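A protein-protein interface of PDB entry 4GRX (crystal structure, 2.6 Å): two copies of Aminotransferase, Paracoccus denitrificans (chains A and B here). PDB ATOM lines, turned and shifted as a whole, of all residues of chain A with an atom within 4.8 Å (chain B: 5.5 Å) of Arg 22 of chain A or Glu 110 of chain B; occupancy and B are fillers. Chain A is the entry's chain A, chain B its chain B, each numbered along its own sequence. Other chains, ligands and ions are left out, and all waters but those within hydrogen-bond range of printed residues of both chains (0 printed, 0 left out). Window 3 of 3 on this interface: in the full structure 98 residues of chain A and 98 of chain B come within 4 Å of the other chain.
No position is printed for both chains.
The backbone carbonyl oxygen (O) of Thr 105 of chain B lies within hydrogen-bond range of the side-chain hydroxyl (OG) of Ser 109 of chain B.
The side-chain carboxylate of Glu 110 of chain B is in salt-bridge range of the guanidinium group of Arg 22 of chain A (3.4 Å).
Printed residues of chain A that touch a printed residue of chain B: Trp 19, Arg 22, Ala 23 and Tyr 26.
Hydrophobic or aromatic side chains of chain A that line the printed part of chain B: Trp 19, Ala 23 and Tyr 26.
Of the 11 printed residues of chain B, 5 touch a printed residue of chain A.
Among the printed residues, 8 pairs touch across the chains.
Among the printed residues, Asp or Glu carboxylates within 4 Å of a Lys or Arg side-chain nitrogen of the other chain: Arg 22 of chain A with Glu 110 of chain B (3.4 Å).
CG1 of Val 106 of chain B touches CE3 of Trp 19 of chain A (3.9 Å).
CG1 of Val 106 of chain B touches CB of Arg 22 of chain A, at 3.7 Å.
Arg 22 of chain A touches Met 107 of chain B (NH2 to CG, 3.9 Å).
Val 106 of chain B touches Ala 23 of chain A.
CB of Tyr 26 of chain A touches CB of Ser 109 of chain B, at 3.7 Å.
Glu 110 of chain B touches Tyr 26 of chain A.
Val 113 of chain B touches Tyr 26 of chain A.
Of the printed residues of chain B, Arg 22 of chain A touches Val 106 (3.7 Å), Met 107 (3.9 Å) and Glu 110 (3.4 Å).
Of the printed residues of chain A, Ser 109 of chain B touches Tyr 26.
Of the printed residues of chain B, Ala 23 of chain A touches Val 106 (3.8 Å).
Thr 25 of chain A touches none of the printed residues of chain B.
Ala 21 of chain A touches none of the printed residues of chain B.
The nearest printed residue of chain B that does not touch Arg 22 of chain A is Ser 109 of chain B (6.1 Å).
The nearest printed residue of chain A that does not touch Val 113 of chain B is Thr 25 of chain A (6.1 Å).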
ATOM      1  N   GLN A  17      -0.104   9.776  23.705  1.00  0.00           N
ATOM      2  CA  GLN A  17      -1.137   9.746  22.631  1.00  0.00           C
ATOM      3  C   GLN A  17      -1.207   8.394  21.906  1.00  0.00           C
ATOM      4  O   GLN A  17      -0.431   8.118  20.987  1.00  0.00           O
ATOM      5  CB  GLN A  17      -0.897  10.889  21.634  1.00  0.00           C
ATOM      6  CG  GLN A  17      -1.541  12.221  22.014  1.00  0.00           C
ATOM      7  CD  GLN A  17      -3.027  12.082  22.322  1.00  0.00           C
ATOM      8  OE1 GLN A  17      -3.400  11.565  23.383  1.00  0.00           O
ATOM      9  NE2 GLN A  17      -3.888  12.536  21.391  1.00  0.00           N
ATOM     10  N   SER A  18      -2.145   7.551  22.322  1.00  0.00           N
ATOM     11  CA  SER A  18      -2.347   6.261  21.682  1.00  0.00           C
ATOM     12  C   SER A  18      -2.991   6.426  20.304  1.00  0.00           C
ATOM     13  O   SER A  18      -3.497   7.487  19.966  1.00  0.00           O
ATOM     14  CB  SER A  18      -3.249   5.406  22.552  1.00  0.00           C
ATOM     15  OG  SER A  18      -4.574   5.873  22.450  1.00  0.00           O
ATOM     16  N   TRP A  19      -2.988   5.362  19.514  1.00  0.00           N
ATOM     17  CA  TRP A  19      -3.630   5.397  18.213  1.00  0.00           C
ATOM     18  C   TRP A  19      -5.109   5.571  18.363  1.00  0.00           C
ATOM     19  O   TRP A  19      -5.726   6.349  17.644  1.00  0.00           O
ATOM     20  CB  TRP A  19      -3.323   4.131  17.445  1.00  0.00           C
ATOM     21  CG  TRP A  19      -1.928   4.126  16.896  1.00  0.00           C
ATOM     22  CD1 TRP A  19      -0.816   3.469  17.408  1.00  0.00           C
ATOM     23  CD2 TRP A  19      -1.441   4.827  15.701  1.00  0.00           C
ATOM     24  NE1 TRP A  19       0.287   3.700  16.630  1.00  0.00           N
ATOM     25  CE2 TRP A  19      -0.012   4.507  15.595  1.00  0.00           C
ATOM     26  CE3 TRP A  19      -2.021   5.653  14.744  1.00  0.00           C
ATOM     27  CZ2 TRP A  19       0.781   5.004  14.567  1.00  0.00           C
ATOM     28  CZ3 TRP A  19      -1.209   6.145  13.708  1.00  0.00           C
ATOM     29  CH2 TRP A  19       0.164   5.832  13.630  1.00  0.00           C
ATOM     30  N   GLU A  20      -5.688   4.852  19.318  1.00  0.00           N
ATOM     31  CA  GLU A  20      -7.109   4.956  19.613  1.00  0.00           C
ATOM     32  C   GLU A  20      -7.456   6.392  20.001  1.00  0.00           C
ATOM     33  O   GLU A  20      -8.443   6.946  19.522  1.00  0.00           O
ATOM     34  CB  GLU A  20      -7.500   3.979  20.727  1.00  0.00           C
ATOM     35  CG  GLU A  20      -7.378   2.507  20.355  1.00  0.00           C
ATOM     36  CD  GLU A  20      -5.961   1.945  20.473  1.00  0.00           C
ATOM     37  OE1 GLU A  20      -5.030   2.658  20.930  1.00  0.00           O
ATOM     38  OE2 GLU A  20      -5.783   0.760  20.105  1.00  0.00           O
ATOM     39  N   ALA A  21      -6.630   6.998  20.851  1.00  0.00           N
ATOM     40  CA  ALA A  21      -6.899   8.353  21.298  1.00  0.00           C
ATOM     41  C   ALA A  21      -6.851   9.313  20.121  1.00  0.00           C
ATOM     42  O   ALA A  21      -7.822  10.022  19.865  1.00  0.00           O
ATOM     43  CB  ALA A  21      -5.925   8.771  22.377  1.00  0.00           C
ATOM     44  N   ARG A  22      -5.730   9.314  19.403  1.00  0.00           N
ATOM     45  CA  ARG A  22      -5.561  10.140  18.209  1.00  0.00           C
ATOM     46  C   ARG A  22      -6.720  10.021  17.212  1.00  0.00           C
ATOM     47  O   ARG A  22      -7.206  11.035  16.694  1.00  0.00           O
ATOM     48  CB  ARG A  22      -4.211   9.859  17.537  1.00  0.00           C
ATOM     49  CG  ARG A  22      -3.036  10.402  18.340  1.00  0.00           C
ATOM     50  CD  ARG A  22      -1.754   9.629  18.112  1.00  0.00           C
ATOM     51  NE  ARG A  22      -1.151   9.932  16.821  1.00  0.00           N
ATOM     52  CZ  ARG A  22      -0.265   9.145  16.207  1.00  0.00           C
ATOM     53  NH1 ARG A  22       0.120   7.989  16.769  1.00  0.00           N
ATOM     54  NH2 ARG A  22       0.232   9.506  15.025  1.00  0.00           N
ATOM     55  N   ALA A  23      -7.184   8.796  16.976  1.00  0.00           N
ATOM     56  CA  ALA A  23      -8.289   8.568  16.054  1.00  0.00           C
ATOM     57  C   ALA A  23      -9.562   9.269  16.513  1.00  0.00           C
ATOM     58  O   ALA A  23     -10.190   9.947  15.722  1.00  0.00           O
ATOM     59  CB  ALA A  23      -8.516   7.082  15.835  1.00  0.00           C
ATOM     60  N   GLU A  24      -9.909   9.145  17.794  1.00  0.00           N
ATOM     61  CA  GLU A  24     -11.133   9.748  18.347  1.00  0.00           C
ATOM     62  C   GLU A  24     -11.105  11.270  18.313  1.00  0.00           C
ATOM     63  O   GLU A  24     -12.132  11.909  18.095  1.00  0.00           O
ATOM     64  CB  GLU A  24     -11.378   9.274  19.785  1.00  0.00           C
ATOM     65  CG  GLU A  24     -12.850   9.186  20.176  1.00  0.00           C
ATOM     66  CD  GLU A  24     -13.155   8.076  21.206  1.00  0.00           C
ATOM     67  OE1 GLU A  24     -13.057   6.849  20.873  1.00  0.00           O
ATOM     68  OE2 GLU A  24     -13.531   8.437  22.354  1.00  0.00           O
ATOM     69  N   THR A  25      -9.920  11.828  18.513  1.00  0.00           N
ATOM     70  CA  THR A  25      -9.719  13.252  18.629  1.00  0.00           C
ATOM     71  C   THR A  25      -9.944  14.023  17.331  1.00  0.00           C
ATOM     72  O   THR A  25     -10.430  15.152  17.364  1.00  0.00           O
ATOM     73  CB  THR A  25      -8.296  13.542  19.156  1.00  0.00           C
ATOM     74  OG1 THR A  25      -8.136  12.928  20.438  1.00  0.00           O
ATOM     75  CG2 THR A  25      -8.040  15.027  19.299  1.00  0.00           C
ATOM     76  N   TYR A  26      -9.598  13.422  16.189  1.00  0.00           N
ATOM     77  CA  TYR A  26      -9.530  14.173  14.930  1.00  0.00           C
ATOM     78  C   TYR A  26     -10.494  13.682  13.854  1.00  0.00           C
ATOM     79  O   TYR A  26     -10.779  14.403  12.888  1.00  0.00           O
ATOM     80  CB  TYR A  26      -8.096  14.195  14.385  1.00  0.00           C
ATOM     81  CG  TYR A  26      -7.082  14.820  15.321  1.00  0.00           C
ATOM     82  CD1 TYR A  26      -6.206  14.027  16.066  1.00  0.00           C
ATOM     83  CD2 TYR A  26      -7.006  16.204  15.471  1.00  0.00           C
ATOM     84  CE1 TYR A  26      -5.281  14.600  16.929  1.00  0.00           C
ATOM     85  CE2 TYR A  26      -6.082  16.782  16.328  1.00  0.00           C
ATOM     86  CZ  TYR A  26      -5.227  15.980  17.051  1.00  0.00           C
ATOM     87  OH  TYR A  26      -4.320  16.562  17.897  1.00  0.00           O
ATOM     88  N   THR B 105      -4.422   7.215   7.734  1.00  0.00           N
ATOM     89  CA  THR B 105      -5.635   7.996   7.928  1.00  0.00           C
ATOM     90  C   THR B 105      -5.556   8.844   9.190  1.00  0.00           C
ATOM     91  O   THR B 105      -5.824  10.034   9.152  1.00  0.00           O
ATOM     92  CB  THR B 105      -6.895   7.111   7.939  1.00  0.00           C
ATOM     93  OG1 THR B 105      -6.832   6.178   6.847  1.00  0.00           O
ATOM     94  CG2 THR B 105      -8.148   7.970   7.785  1.00  0.00           C
ATOM     95  N   VAL B 106      -5.153   8.228  10.293  1.00  0.00           N
ATOM     96  CA  VAL B 106      -5.093   8.900  11.584  1.00  0.00           C
ATOM     97  C   VAL B 106      -4.019   9.999  11.593  1.00  0.00           C
ATOM     98  O   VAL B 106      -4.234  11.075  12.151  1.00  0.00           O
ATOM     99  CB  VAL B 106      -4.905   7.864  12.720  1.00  0.00           C
ATOM    100  CG1 VAL B 106      -4.632   8.511  14.075  1.00  0.00           C
ATOM    101  CG2 VAL B 106      -6.137   6.980  12.815  1.00  0.00           C
ATOM    102  N   MET B 107      -2.878   9.746  10.956  1.00  0.00           N
ATOM    103  CA  MET B 107      -1.824  10.749  10.878  1.00  0.00           C
ATOM    104  C   MET B 107      -2.338  11.966  10.102  1.00  0.00           C
ATOM    105  O   MET B 107      -2.227  13.102  10.582  1.00  0.00           O
ATOM    106  CB  MET B 107      -0.543  10.169  10.269  1.00  0.00           C
ATOM    107  CG  MET B 107       0.114   9.079  11.118  1.00  0.00           C
ATOM    108  SD  MET B 107       1.365   8.072  10.263  1.00  0.00           S
ATOM    109  CE  MET B 107       2.718   9.242  10.112  1.00  0.00           C
ATOM    110  N   LEU B 108      -2.961  11.733   8.946  1.00  0.00           N
ATOM    111  CA  LEU B 108      -3.490  12.835   8.151  1.00  0.00           C
ATOM    112  C   LEU B 108      -4.541  13.685   8.853  1.00  0.00           C
ATOM    113  O   LEU B 108      -4.526  14.911   8.728  1.00  0.00           O
ATOM    114  CB  LEU B 108      -4.026  12.373   6.809  1.00  0.00           C
ATOM    115  CG  LEU B 108      -4.403  13.552   5.907  1.00  0.00           C
ATOM    116  CD1 LEU B 108      -3.164  14.376   5.595  1.00  0.00           C
ATOM    117  CD2 LEU B 108      -5.069  13.075   4.634  1.00  0.00           C
ATOM    118  N   SER B 109      -5.448  13.067   9.598  1.00  0.00           N
ATOM    119  CA  SER B 109      -6.483  13.859  10.256  1.00  0.00           C
ATOM    120  C   SER B 109      -5.811  14.792  11.256  1.00  0.00           C
ATOM    121  O   SER B 109      -6.120  15.983  11.306  1.00  0.00           O
ATOM    122  CB  SER B 109      -7.540  12.970  10.905  1.00  0.00           C
ATOM    123  OG  SER B 109      -8.108  12.097   9.943  1.00  0.00           O
ATOM    124  N   GLU B 110      -4.854  14.236  12.000  1.00  0.00           N
ATOM    125  CA  GLU B 110      -4.036  14.981  12.941  1.00  0.00           C
ATOM    126  C   GLU B 110      -3.362  16.149  12.235  1.00  0.00           C
ATOM    127  O   GLU B 110      -3.394  17.282  12.707  1.00  0.00           O
ATOM    128  CB  GLU B 110      -2.973  14.051  13.569  1.00  0.00           C
ATOM    129  CG  GLU B 110      -2.418  14.522  14.902  1.00  0.00           C
ATOM    130  CD  GLU B 110      -1.495  13.508  15.592  1.00  0.00           C
ATOM    131  OE1 GLU B 110      -0.585  12.958  14.918  1.00  0.00           O
ATOM    132  OE2 GLU B 110      -1.661  13.276  16.826  1.00  0.00           O
ATOM    133  N   LYS B 111      -2.754  15.864  11.092  1.00  0.00           N
ATOM    134  CA  LYS B 111      -1.954  16.860  10.401  1.00  0.00           C
ATOM    135  C   LYS B 111      -2.847  17.918   9.751  1.00  0.00           C
ATOM    136  O   LYS B 111      -2.465  19.078   9.678  1.00  0.00           O
ATOM    137  CB  LYS B 111      -1.021  16.177   9.393  1.00  0.00           C
ATOM    138  CG  LYS B 111      -0.261  17.077   8.410  1.00  0.00           C
ATOM    139  CD  LYS B 111       0.740  17.987   9.101  1.00  0.00           C
ATOM    140  CE  LYS B 111       1.695  17.181   9.961  1.00  0.00           C
ATOM    141  NZ  LYS B 111       2.554  18.126  10.696  1.00  0.00           N
ATOM    142  N   LEU B 112      -4.048  17.538   9.322  1.00  0.00           N
ATOM    143  CA  LEU B 112      -4.938  18.518   8.730  1.00  0.00           C
ATOM    144  C   LEU B 112      -5.489  19.532   9.738  1.00  0.00           C
ATOM    145  O   LEU B 112      -5.578  20.730   9.433  1.00  0.00           O
ATOM    146  CB  LEU B 112      -6.055  17.858   7.934  1.00  0.00           C
ATOM    147  CG  LEU B 112      -5.624  17.326   6.566  1.00  0.00           C
ATOM    148  CD1 LEU B 112      -6.788  16.628   5.880  1.00  0.00           C
ATOM    149  CD2 LEU B 112      -5.029  18.414   5.675  1.00  0.00           C
ATOM    150  N   VAL B 113      -5.829  19.068  10.938  1.00  0.00           N
ATOM    151  CA  VAL B 113      -6.237  19.988  11.999  1.00  0.00           C
ATOM    152  C   VAL B 113      -5.101  20.948  12.385  1.00  0.00           C
ATOM    153  O   VAL B 113      -5.314  22.149  12.525  1.00  0.00           O
ATOM    154  CB  VAL B 113      -6.775  19.225  13.219  1.00  0.00           C
ATOM    155  CG1 VAL B 113      -6.919  20.149  14.431  1.00  0.00           C
ATOM    156  CG2 VAL B 113      -8.096  18.565  12.853  1.00  0.00           C
ATOM    157  N   GLU B 114      -3.892  20.415  12.531  1.00  0.00           N
ATOM    158  CA  GLU B 114      -2.738  21.233  12.894  1.00  0.00           C
ATOM    159  C   GLU B 114      -2.525  22.327  11.827  1.00  0.00           C
ATOM    160  O   GLU B 114      -2.624  23.516  12.111  1.00  0.00           O
ATOM    161  CB  GLU B 114      -1.499  20.345  13.066  1.00  0.00           C
ATOM    162  CG  GLU B 114      -0.254  21.020  13.626  1.00  0.00           C
ATOM    163  CD  GLU B 114       1.045  20.442  13.043  1.00  0.00           C
ATOM    164  OE1 GLU B 114       2.108  21.116  13.114  1.00  0.00           O
ATOM    165  OE2 GLU B 114       1.016  19.314  12.499  1.00  0.00           O
ATOM    166  N   VAL B 115      -2.316  21.894  10.594  1.00  0.00           N
ATOM    167  CA  VAL B 115      -2.050  22.737   9.441  1.00  0.00           C
ATOM    168  C   VAL B 115      -3.206  23.683   9.038  1.00  0.00           C
ATOM    169  O   VAL B 115      -2.988  24.661   8.311  1.00  0.00           O
ATOM    170  CB  VAL B 115      -1.638  21.807   8.283  1.00  0.00           C
ATOM    171  CG1 VAL B 115      -2.213  22.238   6.961  1.00  0.00           C
ATOM    172  CG2 VAL B 115      -0.130  21.645   8.233  1.00  0.00           C
